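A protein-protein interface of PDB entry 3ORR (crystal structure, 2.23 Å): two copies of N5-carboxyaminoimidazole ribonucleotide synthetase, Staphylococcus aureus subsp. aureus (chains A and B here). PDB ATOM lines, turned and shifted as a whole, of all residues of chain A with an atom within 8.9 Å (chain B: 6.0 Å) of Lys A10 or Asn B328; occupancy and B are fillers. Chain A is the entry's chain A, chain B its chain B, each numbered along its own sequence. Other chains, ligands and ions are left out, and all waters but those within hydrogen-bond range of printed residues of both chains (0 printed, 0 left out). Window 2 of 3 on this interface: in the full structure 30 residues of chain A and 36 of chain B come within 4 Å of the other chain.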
ATOM      1  N   ASN A   7      24.293  20.908  -4.059  1.00  0.00           N
ATOM      2  CA  ASN A   7      22.921  20.469  -4.317  1.00  0.00           C
ATOM      3  C   ASN A   7      22.088  20.260  -3.092  1.00  0.00           C
ATOM      4  O   ASN A   7      22.519  19.608  -2.124  1.00  0.00           O
ATOM      5  CB  ASN A   7      22.945  19.192  -5.109  1.00  0.00           C
ATOM      6  CG  ASN A   7      23.687  19.348  -6.402  1.00  0.00           C
ATOM      7  OD1 ASN A   7      24.201  20.434  -6.706  1.00  0.00           O
ATOM      8  ND2 ASN A   7      23.779  18.277  -7.162  1.00  0.00           N
ATOM      9  N   LYS A   8      20.911  20.854  -3.135  1.00  0.00           N
ATOM     10  CA  LYS A   8      19.915  20.695  -2.100  1.00  0.00           C
ATOM     11  C   LYS A   8      19.104  19.490  -2.499  1.00  0.00           C
ATOM     12  O   LYS A   8      18.362  19.521  -3.488  1.00  0.00           O
ATOM     13  CB  LYS A   8      19.053  21.945  -1.978  1.00  0.00           C
ATOM     14  CG  LYS A   8      19.831  23.114  -1.318  1.00  0.00           C
ATOM     15  CD  LYS A   8      18.962  24.381  -1.204  1.00  0.00           C
ATOM     16  CE  LYS A   8      19.723  25.525  -0.493  1.00  0.00           C
ATOM     17  NZ  LYS A   8      19.087  26.863  -0.591  1.00  0.00           N
ATOM     18  N   LEU A   9      19.290  18.400  -1.769  1.00  0.00           N
ATOM     19  CA  LEU A   9      18.620  17.154  -2.112  1.00  0.00           C
ATOM     20  C   LEU A   9      17.424  17.027  -1.195  1.00  0.00           C
ATOM     21  O   LEU A   9      17.543  17.255   0.018  1.00  0.00           O
ATOM     22  CB  LEU A   9      19.571  15.983  -1.899  1.00  0.00           C
ATOM     23  CG  LEU A   9      20.888  16.018  -2.661  1.00  0.00           C
ATOM     24  CD1 LEU A   9      21.684  14.799  -2.233  1.00  0.00           C
ATOM     25  CD2 LEU A   9      20.615  15.996  -4.192  1.00  0.00           C
ATOM     26  N   LYS A  10      16.281  16.645  -1.739  1.00  0.00           N
ATOM     27  CA  LYS A  10      15.054  16.475  -0.922  1.00  0.00           C
ATOM     28  C   LYS A  10      14.821  15.004  -0.571  1.00  0.00           C
ATOM     29  O   LYS A  10      15.405  14.099  -1.191  1.00  0.00           O
ATOM     30  CB  LYS A  10      13.840  17.003  -1.675  1.00  0.00           C
ATOM     31  CG  LYS A  10      13.783  18.536  -1.820  1.00  0.00           C
ATOM     32  CD  LYS A  10      12.706  18.959  -2.877  1.00  0.00           C
ATOM     33  CE  LYS A  10      12.344  20.456  -2.792  1.00  0.00           C
ATOM     34  NZ  LYS A  10      13.385  21.350  -3.356  1.00  0.00           N
ATOM     35  N   PHE A  11      13.948  14.739   0.398  1.00  0.00           N
ATOM     36  CA  PHE A  11      13.664  13.358   0.741  1.00  0.00           C
ATOM     37  C   PHE A  11      13.391  12.533  -0.528  1.00  0.00           C
ATOM     38  O   PHE A  11      12.837  13.043  -1.532  1.00  0.00           O
ATOM     39  CB  PHE A  11      12.520  13.221   1.755  1.00  0.00           C
ATOM     40  CG  PHE A  11      11.169  13.700   1.235  1.00  0.00           C
ATOM     41  CD1 PHE A  11      10.379  12.872   0.431  1.00  0.00           C
ATOM     42  CD2 PHE A  11      10.688  14.981   1.573  1.00  0.00           C
ATOM     43  CE1 PHE A  11       9.142  13.311  -0.035  1.00  0.00           C
ATOM     44  CE2 PHE A  11       9.454  15.411   1.126  1.00  0.00           C
ATOM     45  CZ  PHE A  11       8.683  14.577   0.314  1.00  0.00           C
ATOM     46  N   GLY A  12      13.776  11.273  -0.473  1.00  0.00           N
ATOM     47  CA  GLY A  12      13.701  10.417  -1.651  1.00  0.00           C
ATOM     48  C   GLY A  12      15.033  10.208  -2.366  1.00  0.00           C
ATOM     49  O   GLY A  12      15.191   9.225  -3.061  1.00  0.00           O
ATOM     50  N   ALA A  13      15.986  11.136  -2.218  1.00  0.00           N
ATOM     51  CA  ALA A  13      17.270  10.981  -2.885  1.00  0.00           C
ATOM     52  C   ALA A  13      18.085   9.943  -2.087  1.00  0.00           C
ATOM     53  O   ALA A  13      17.708   9.581  -0.955  1.00  0.00           O
ATOM     54  CB  ALA A  13      17.985  12.315  -2.959  1.00  0.00           C
ATOM     55  N   THR A  14      19.175   9.449  -2.686  1.00  0.00           N
ATOM     56  CA  THR A  14      19.963   8.399  -2.124  1.00  0.00           C
ATOM     57  C   THR A  14      21.295   8.920  -1.564  1.00  0.00           C
ATOM     58  O   THR A  14      21.979   9.688  -2.210  1.00  0.00           O
ATOM     59  CB  THR A  14      20.222   7.320  -3.173  1.00  0.00           C
ATOM     60  OG1 THR A  14      18.971   6.779  -3.581  1.00  0.00           O
ATOM     61  CG2 THR A  14      21.088   6.214  -2.603  1.00  0.00           C
ATOM     62  N   ILE A  15      21.673   8.436  -0.387  1.00  0.00           N
ATOM     63  CA  ILE A  15      22.918   8.829   0.248  1.00  0.00           C
ATOM     64  C   ILE A  15      23.837   7.606   0.250  1.00  0.00           C
ATOM     65  O   ILE A  15      23.435   6.537   0.708  1.00  0.00           O
ATOM     66  CB  ILE A  15      22.674   9.297   1.699  1.00  0.00           C
ATOM     67  CG1 ILE A  15      21.584  10.414   1.747  1.00  0.00           C
ATOM     68  CG2 ILE A  15      23.971   9.697   2.380  1.00  0.00           C
ATOM     69  CD1 ILE A  15      21.359  11.054   3.171  1.00  0.00           C
ATOM     70  N   ALA A  31      19.305   9.216   8.402  1.00  0.00           N
ATOM     71  CA  ALA A  31      18.887   9.328   7.016  1.00  0.00           C
ATOM     72  C   ALA A  31      17.511   8.675   6.756  1.00  0.00           C
ATOM     73  O   ALA A  31      16.675   9.272   6.104  1.00  0.00           O
ATOM     74  CB  ALA A  31      19.962   8.747   6.067  1.00  0.00           C
ATOM     75  N   MET A  34      14.570  10.417   8.020  1.00  0.00           N
ATOM     76  CA  MET A  34      14.323  11.658   7.259  1.00  0.00           C
ATOM     77  C   MET A  34      13.834  11.393   5.841  1.00  0.00           C
ATOM     78  O   MET A  34      13.716  12.304   5.032  1.00  0.00           O
ATOM     79  CB  MET A  34      15.643  12.490   7.231  1.00  0.00           C
ATOM     80  CG  MET A  34      16.017  12.908   8.700  1.00  0.00           C
ATOM     81  SD  MET A  34      17.876  13.513   8.904  1.00  0.00           S
ATOM     82  CE  MET A  34      17.410  15.179   8.158  1.00  0.00           C
ATOM     83  N   GLY A  35      13.620  10.134   5.519  1.00  0.00           N
ATOM     84  CA  GLY A  35      13.148   9.789   4.194  1.00  0.00           C
ATOM     85  C   GLY A  35      14.250   9.723   3.130  1.00  0.00           C
ATOM     86  O   GLY A  35      13.930   9.789   1.937  1.00  0.00           O
ATOM     87  N   TYR A  36      15.522   9.580   3.529  1.00  0.00           N
ATOM     88  CA  TYR A  36      16.596   9.358   2.520  1.00  0.00           C
ATOM     89  C   TYR A  36      16.929   7.885   2.357  1.00  0.00           C
ATOM     90  O   TYR A  36      16.990   7.165   3.347  1.00  0.00           O
ATOM     91  CB  TYR A  36      17.864  10.151   2.845  1.00  0.00           C
ATOM     92  CG  TYR A  36      17.642  11.649   2.768  1.00  0.00           C
ATOM     93  CD1 TYR A  36      17.635  12.302   1.532  1.00  0.00           C
ATOM     94  CD2 TYR A  36      17.389  12.403   3.919  1.00  0.00           C
ATOM     95  CE1 TYR A  36      17.420  13.686   1.426  1.00  0.00           C
ATOM     96  CE2 TYR A  36      17.198  13.805   3.832  1.00  0.00           C
ATOM     97  CZ  TYR A  36      17.196  14.427   2.581  1.00  0.00           C
ATOM     98  OH  TYR A  36      16.966  15.782   2.452  1.00  0.00           O
ATOM     99  N   LYS A  37      17.177   7.450   1.132  1.00  0.00           N
ATOM    100  CA  LYS A  37      17.693   6.119   0.879  1.00  0.00           C
ATOM    101  C   LYS A  37      19.190   6.028   1.149  1.00  0.00           C
ATOM    102  O   LYS A  37      19.931   7.005   1.004  1.00  0.00           O
ATOM    103  CB  LYS A  37      17.339   5.642  -0.514  1.00  0.00           C
ATOM    104  CG  LYS A  37      15.855   5.779  -0.819  1.00  0.00           C
ATOM    105  CD  LYS A  37      15.540   5.063  -2.156  1.00  0.00           C
ATOM    106  CE  LYS A  37      14.123   5.415  -2.603  1.00  0.00           C
ATOM    107  NZ  LYS A  37      13.119   4.689  -1.795  1.00  0.00           N
ATOM    108  N   ASP A  75      23.008  10.299  -4.858  1.00  0.00           N
ATOM    109  CA  ASP A  75      22.930  11.720  -5.179  1.00  0.00           C
ATOM    110  C   ASP A  75      23.924  12.466  -4.278  1.00  0.00           C
ATOM    111  O   ASP A  75      24.289  13.602  -4.541  1.00  0.00           O
ATOM    112  CB  ASP A  75      21.496  12.233  -4.935  1.00  0.00           C
ATOM    113  CG  ASP A  75      20.452  11.406  -5.685  1.00  0.00           C
ATOM    114  OD1 ASP A  75      20.422  11.511  -6.914  1.00  0.00           O
ATOM    115  OD2 ASP A  75      19.682  10.643  -5.075  1.00  0.00           O
ATOM    116  N   VAL A  76      24.380  11.816  -3.223  1.00  0.00           N
ATOM    117  CA  VAL A  76      25.463  12.389  -2.414  1.00  0.00           C
ATOM    118  C   VAL A  76      26.261  11.246  -1.765  1.00  0.00           C
ATOM    119  O   VAL A  76      25.711  10.157  -1.511  1.00  0.00           O
ATOM    120  CB  VAL A  76      24.912  13.395  -1.358  1.00  0.00           C
ATOM    121  CG1 VAL A  76      23.932  12.708  -0.370  1.00  0.00           C
ATOM    122  CG2 VAL A  76      26.008  14.041  -0.615  1.00  0.00           C
ATOM    123  N   THR A 299      23.087  16.948   2.707  1.00  0.00           N
ATOM    124  CA  THR A 299      22.023  17.031   1.716  1.00  0.00           C
ATOM    125  C   THR A 299      21.664  18.476   1.360  1.00  0.00           C
ATOM    126  O   THR A 299      20.765  18.699   0.516  1.00  0.00           O
ATOM    127  CB  THR A 299      20.699  16.325   2.197  1.00  0.00           C
ATOM    128  OG1 THR A 299      20.252  16.898   3.438  1.00  0.00           O
ATOM    129  CG2 THR A 299      20.912  14.775   2.366  1.00  0.00           C
ATOM    130  N   GLY A 300      22.316  19.432   2.049  1.00  0.00           N
ATOM    131  CA  GLY A 300      22.265  20.838   1.671  1.00  0.00           C
ATOM    132  C   GLY A 300      21.117  21.615   2.303  1.00  0.00           C
ATOM    133  O   GLY A 300      20.707  22.659   1.804  1.00  0.00           O
ATOM    134  N   GLN A 301      20.579  21.096   3.391  1.00  0.00           N
ATOM    135  CA  GLN A 301      19.437  21.728   4.057  1.00  0.00           C
ATOM    136  C   GLN A 301      19.959  22.787   4.984  1.00  0.00           C
ATOM    137  O   GLN A 301      21.138  22.776   5.302  1.00  0.00           O
ATOM    138  CB  GLN A 301      18.710  20.692   4.908  1.00  0.00           C
ATOM    139  CG  GLN A 301      18.536  19.357   4.233  1.00  0.00           C
ATOM    140  CD  GLN A 301      17.599  19.459   3.102  1.00  0.00           C
ATOM    141  OE1 GLN A 301      16.481  19.962   3.238  1.00  0.00           O
ATOM    142  NE2 GLN A 301      18.033  18.996   1.950  1.00  0.00           N
ATOM    143  N   LEU B 323       2.298  17.438   2.044  1.00  0.00           N
ATOM    144  CA  LEU B 323       3.550  17.413   1.372  1.00  0.00           C
ATOM    145  C   LEU B 323       3.426  18.293   0.138  1.00  0.00           C
ATOM    146  O   LEU B 323       4.281  19.162  -0.098  1.00  0.00           O
ATOM    147  CB  LEU B 323       3.945  15.972   0.970  1.00  0.00           C
ATOM    148  CG  LEU B 323       4.384  14.970   2.077  1.00  0.00           C
ATOM    149  CD1 LEU B 323       4.996  13.711   1.478  1.00  0.00           C
ATOM    150  CD2 LEU B 323       5.385  15.581   3.085  1.00  0.00           C
ATOM    151  N   LEU B 325       1.701  20.759  -0.256  1.00  0.00           N
ATOM    152  CA  LEU B 325       1.736  22.154   0.135  1.00  0.00           C
ATOM    153  C   LEU B 325       3.107  22.656   0.603  1.00  0.00           C
ATOM    154  O   LEU B 325       3.545  23.760   0.206  1.00  0.00           O
ATOM    155  CB  LEU B 325       0.694  22.424   1.201  1.00  0.00           C
ATOM    156  CG  LEU B 325       0.608  23.854   1.758  1.00  0.00           C
ATOM    157  CD1 LEU B 325       0.120  24.924   0.653  1.00  0.00           C
ATOM    158  CD2 LEU B 325      -0.339  23.868   2.997  1.00  0.00           C
ATOM    159  N   LEU B 326       3.766  21.861   1.439  1.00  0.00           N
ATOM    160  CA  LEU B 326       4.877  22.363   2.244  1.00  0.00           C
ATOM    161  C   LEU B 326       6.280  21.827   1.878  1.00  0.00           C
ATOM    162  O   LEU B 326       7.296  22.345   2.369  1.00  0.00           O
ATOM    163  CB  LEU B 326       4.606  22.026   3.728  1.00  0.00           C
ATOM    164  CG  LEU B 326       3.336  22.584   4.375  1.00  0.00           C
ATOM    165  CD1 LEU B 326       3.099  21.903   5.728  1.00  0.00           C
ATOM    166  CD2 LEU B 326       3.345  24.132   4.519  1.00  0.00           C
ATOM    167  N   GLU B 327       6.342  20.770   1.072  1.00  0.00           N
ATOM    168  CA  GLU B 327       7.621  20.051   0.921  1.00  0.00           C
ATOM    169  C   GLU B 327       8.766  20.969   0.486  1.00  0.00           C
ATOM    170  O   GLU B 327       9.896  20.758   0.870  1.00  0.00           O
ATOM    171  CB  GLU B 327       7.510  18.808  -0.021  1.00  0.00           C
ATOM    172  CG  GLU B 327       6.999  19.126  -1.384  1.00  0.00           C
ATOM    173  CD  GLU B 327       6.780  17.893  -2.254  1.00  0.00           C
ATOM    174  OE1 GLU B 327       7.429  16.860  -1.999  1.00  0.00           O
ATOM    175  OE2 GLU B 327       5.978  17.950  -3.209  1.00  0.00           O
ATOM    176  N   ASN B 328       8.465  21.965  -0.317  1.00  0.00           N
ATOM    177  CA  ASN B 328       9.501  22.929  -0.803  1.00  0.00           C
ATOM    178  C   ASN B 328      10.063  23.874   0.267  1.00  0.00           C
ATOM    179  O   ASN B 328      11.162  24.348   0.105  1.00  0.00           O
ATOM    180  CB  ASN B 328       9.012  23.709  -2.032  1.00  0.00           C
ATOM    181  CG  ASN B 328       8.869  22.810  -3.250  1.00  0.00           C
ATOM    182  OD1 ASN B 328       9.482  21.741  -3.325  1.00  0.00           O
ATOM    183  ND2 ASN B 328       8.040  23.213  -4.185  1.00  0.00           N
ATOM    184  N   GLU B 329       9.303  24.101   1.341  1.00  0.00           N
ATOM    185  CA  GLU B 329       9.762  24.821   2.549  1.00  0.00           C
ATOM    186  C   GLU B 329      10.628  23.997   3.520  1.00  0.00           C
ATOM    187  O   GLU B 329      11.328  24.581   4.341  1.00  0.00           O
ATOM    188  CB  GLU B 329       8.581  25.378   3.366  1.00  0.00           C
ATOM    189  CG  GLU B 329       7.470  25.919   2.549  1.00  0.00           C
ATOM    190  CD  GLU B 329       6.555  26.817   3.338  1.00  0.00           C
ATOM    191  OE1 GLU B 329       6.903  27.149   4.481  1.00  0.00           O
ATOM    192  OE2 GLU B 329       5.511  27.218   2.787  1.00  0.00           O
ATOM    193  N   PHE B 330      10.566  22.661   3.447  1.00  0.00           N
ATOM    194  CA  PHE B 330      11.251  21.807   4.442  1.00  0.00           C
ATOM    195  C   PHE B 330      12.723  22.190   4.697  1.00  0.00           C
ATOM    196  O   PHE B 330      13.166  22.214   5.853  1.00  0.00           O
ATOM    197  CB  PHE B 330      11.162  20.308   4.093  1.00  0.00           C
ATOM    198  CG  PHE B 330       9.751  19.700   4.247  1.00  0.00           C
ATOM    199  CD1 PHE B 330       8.766  20.346   4.984  1.00  0.00           C
ATOM    200  CD2 PHE B 330       9.428  18.478   3.627  1.00  0.00           C
ATOM    201  CE1 PHE B 330       7.487  19.784   5.126  1.00  0.00           C
ATOM    202  CE2 PHE B 330       8.166  17.882   3.782  1.00  0.00           C
ATOM    203  CZ  PHE B 330       7.184  18.541   4.498  1.00  0.00           C
ATOM    204  N   ASN B 331      13.477  22.443   3.633  1.00  0.00           N
ATOM    205  CA  ASN B 331      14.891  22.726   3.757  1.00  0.00           C
ATOM    206  C   ASN B 331      15.239  23.913   4.676  1.00  0.00           C
ATOM    207  O   ASN B 331      16.320  23.951   5.249  1.00  0.00           O
ATOM    208  CB  ASN B 331      15.509  22.979   2.366  1.00  0.00           C
ATOM    209  CG  ASN B 331      14.979  24.209   1.759  1.00  0.00           C
ATOM    210  OD1 ASN B 331      13.849  24.227   1.259  1.00  0.00           O
ATOM    211  ND2 ASN B 331      15.744  25.282   1.835  1.00  0.00           N
ATOM    212  N   GLU B 332      14.325  24.870   4.775  1.00  0.00           N
ATOM    213  CA  GLU B 332      14.517  26.086   5.566  1.00  0.00           C
ATOM    214  C   GLU B 332      14.173  25.884   7.027  1.00  0.00           C
ATOM    215  O   GLU B 332      14.413  26.760   7.836  1.00  0.00           O
ATOM    216  CB  GLU B 332      13.642  27.234   5.029  1.00  0.00           C
ATOM    217  CG  GLU B 332      13.967  27.700   3.585  1.00  0.00           C
ATOM    218  CD  GLU B 332      12.969  28.791   3.052  1.00  0.00           C
ATOM    219  OE1 GLU B 332      13.390  29.960   2.938  1.00  0.00           O
ATOM    220  OE2 GLU B 332      11.772  28.498   2.781  1.00  0.00           O
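The side-chain amide nitrogen (NE2) of Gln A301 is in hydrogen-bond range of the backbone carbonyl oxygen (O) of Leu A9 (2.6 Å). OH of Tyr A36 sits at hydrogen-bond distance from NE2 of Gln A301. The side-chain amide nitrogen (NE2) of Gln A301 sits at hydrogen-bond distance from the backbone carbonyl oxygen (O) of Thr A299 (3.1 Å). O of Asn B328 lies close to OD1 of Asn B331.
Among the printed residues, pairs that only touch across the chains: Lys A10 with Asn B328 (3.2 Å), Phe A11 with Leu B323 (3.96 Å), Phe A11 with Glu B327 (3.5 Å), Phe A11 with Phe B330 (3.8 Å) and Gln A301 with Asn B331 (3.2 Å).
Lys A10 touches just one residue of chain B: Asn B328 (3.2 Å). Of the printed residues of chain B, Gln A301 touches Asn B331. Printed residues of chain A within 4 Å of Leu B323: Phe A11. Printed residues of chain A within 4 Å of Glu B327: Phe A11 (3.5 Å). Of chain A, only Lys A10 (3.2 Å) comes within 4 Å of Asn B328. Printed residues of chain A within 4 Å of Phe B330: Phe A11 (3.8 Å). Printed residues of chain A within 4 Å of Asn B331: Gln A301. The nearest residue of chain B that does not touch Lys A10 is Glu B327 (4.4 Å). The nearest printed residue of chain A that does not touch Asn B331 is Lys A8 (4.4 Å).
Along chain B the printed residues that touch a printed residue of chain A span positions 323 to 331. Printed residues of chain A that touch a printed residue of chain B: Lys A10, Phe A11 and Gln A301. Hydrophobic or aromatic side chains of chain A that line the printed part of chain B: Phe A11. Among the printed residues, 5 pairs touch across the chains.
No position is printed for both chains.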
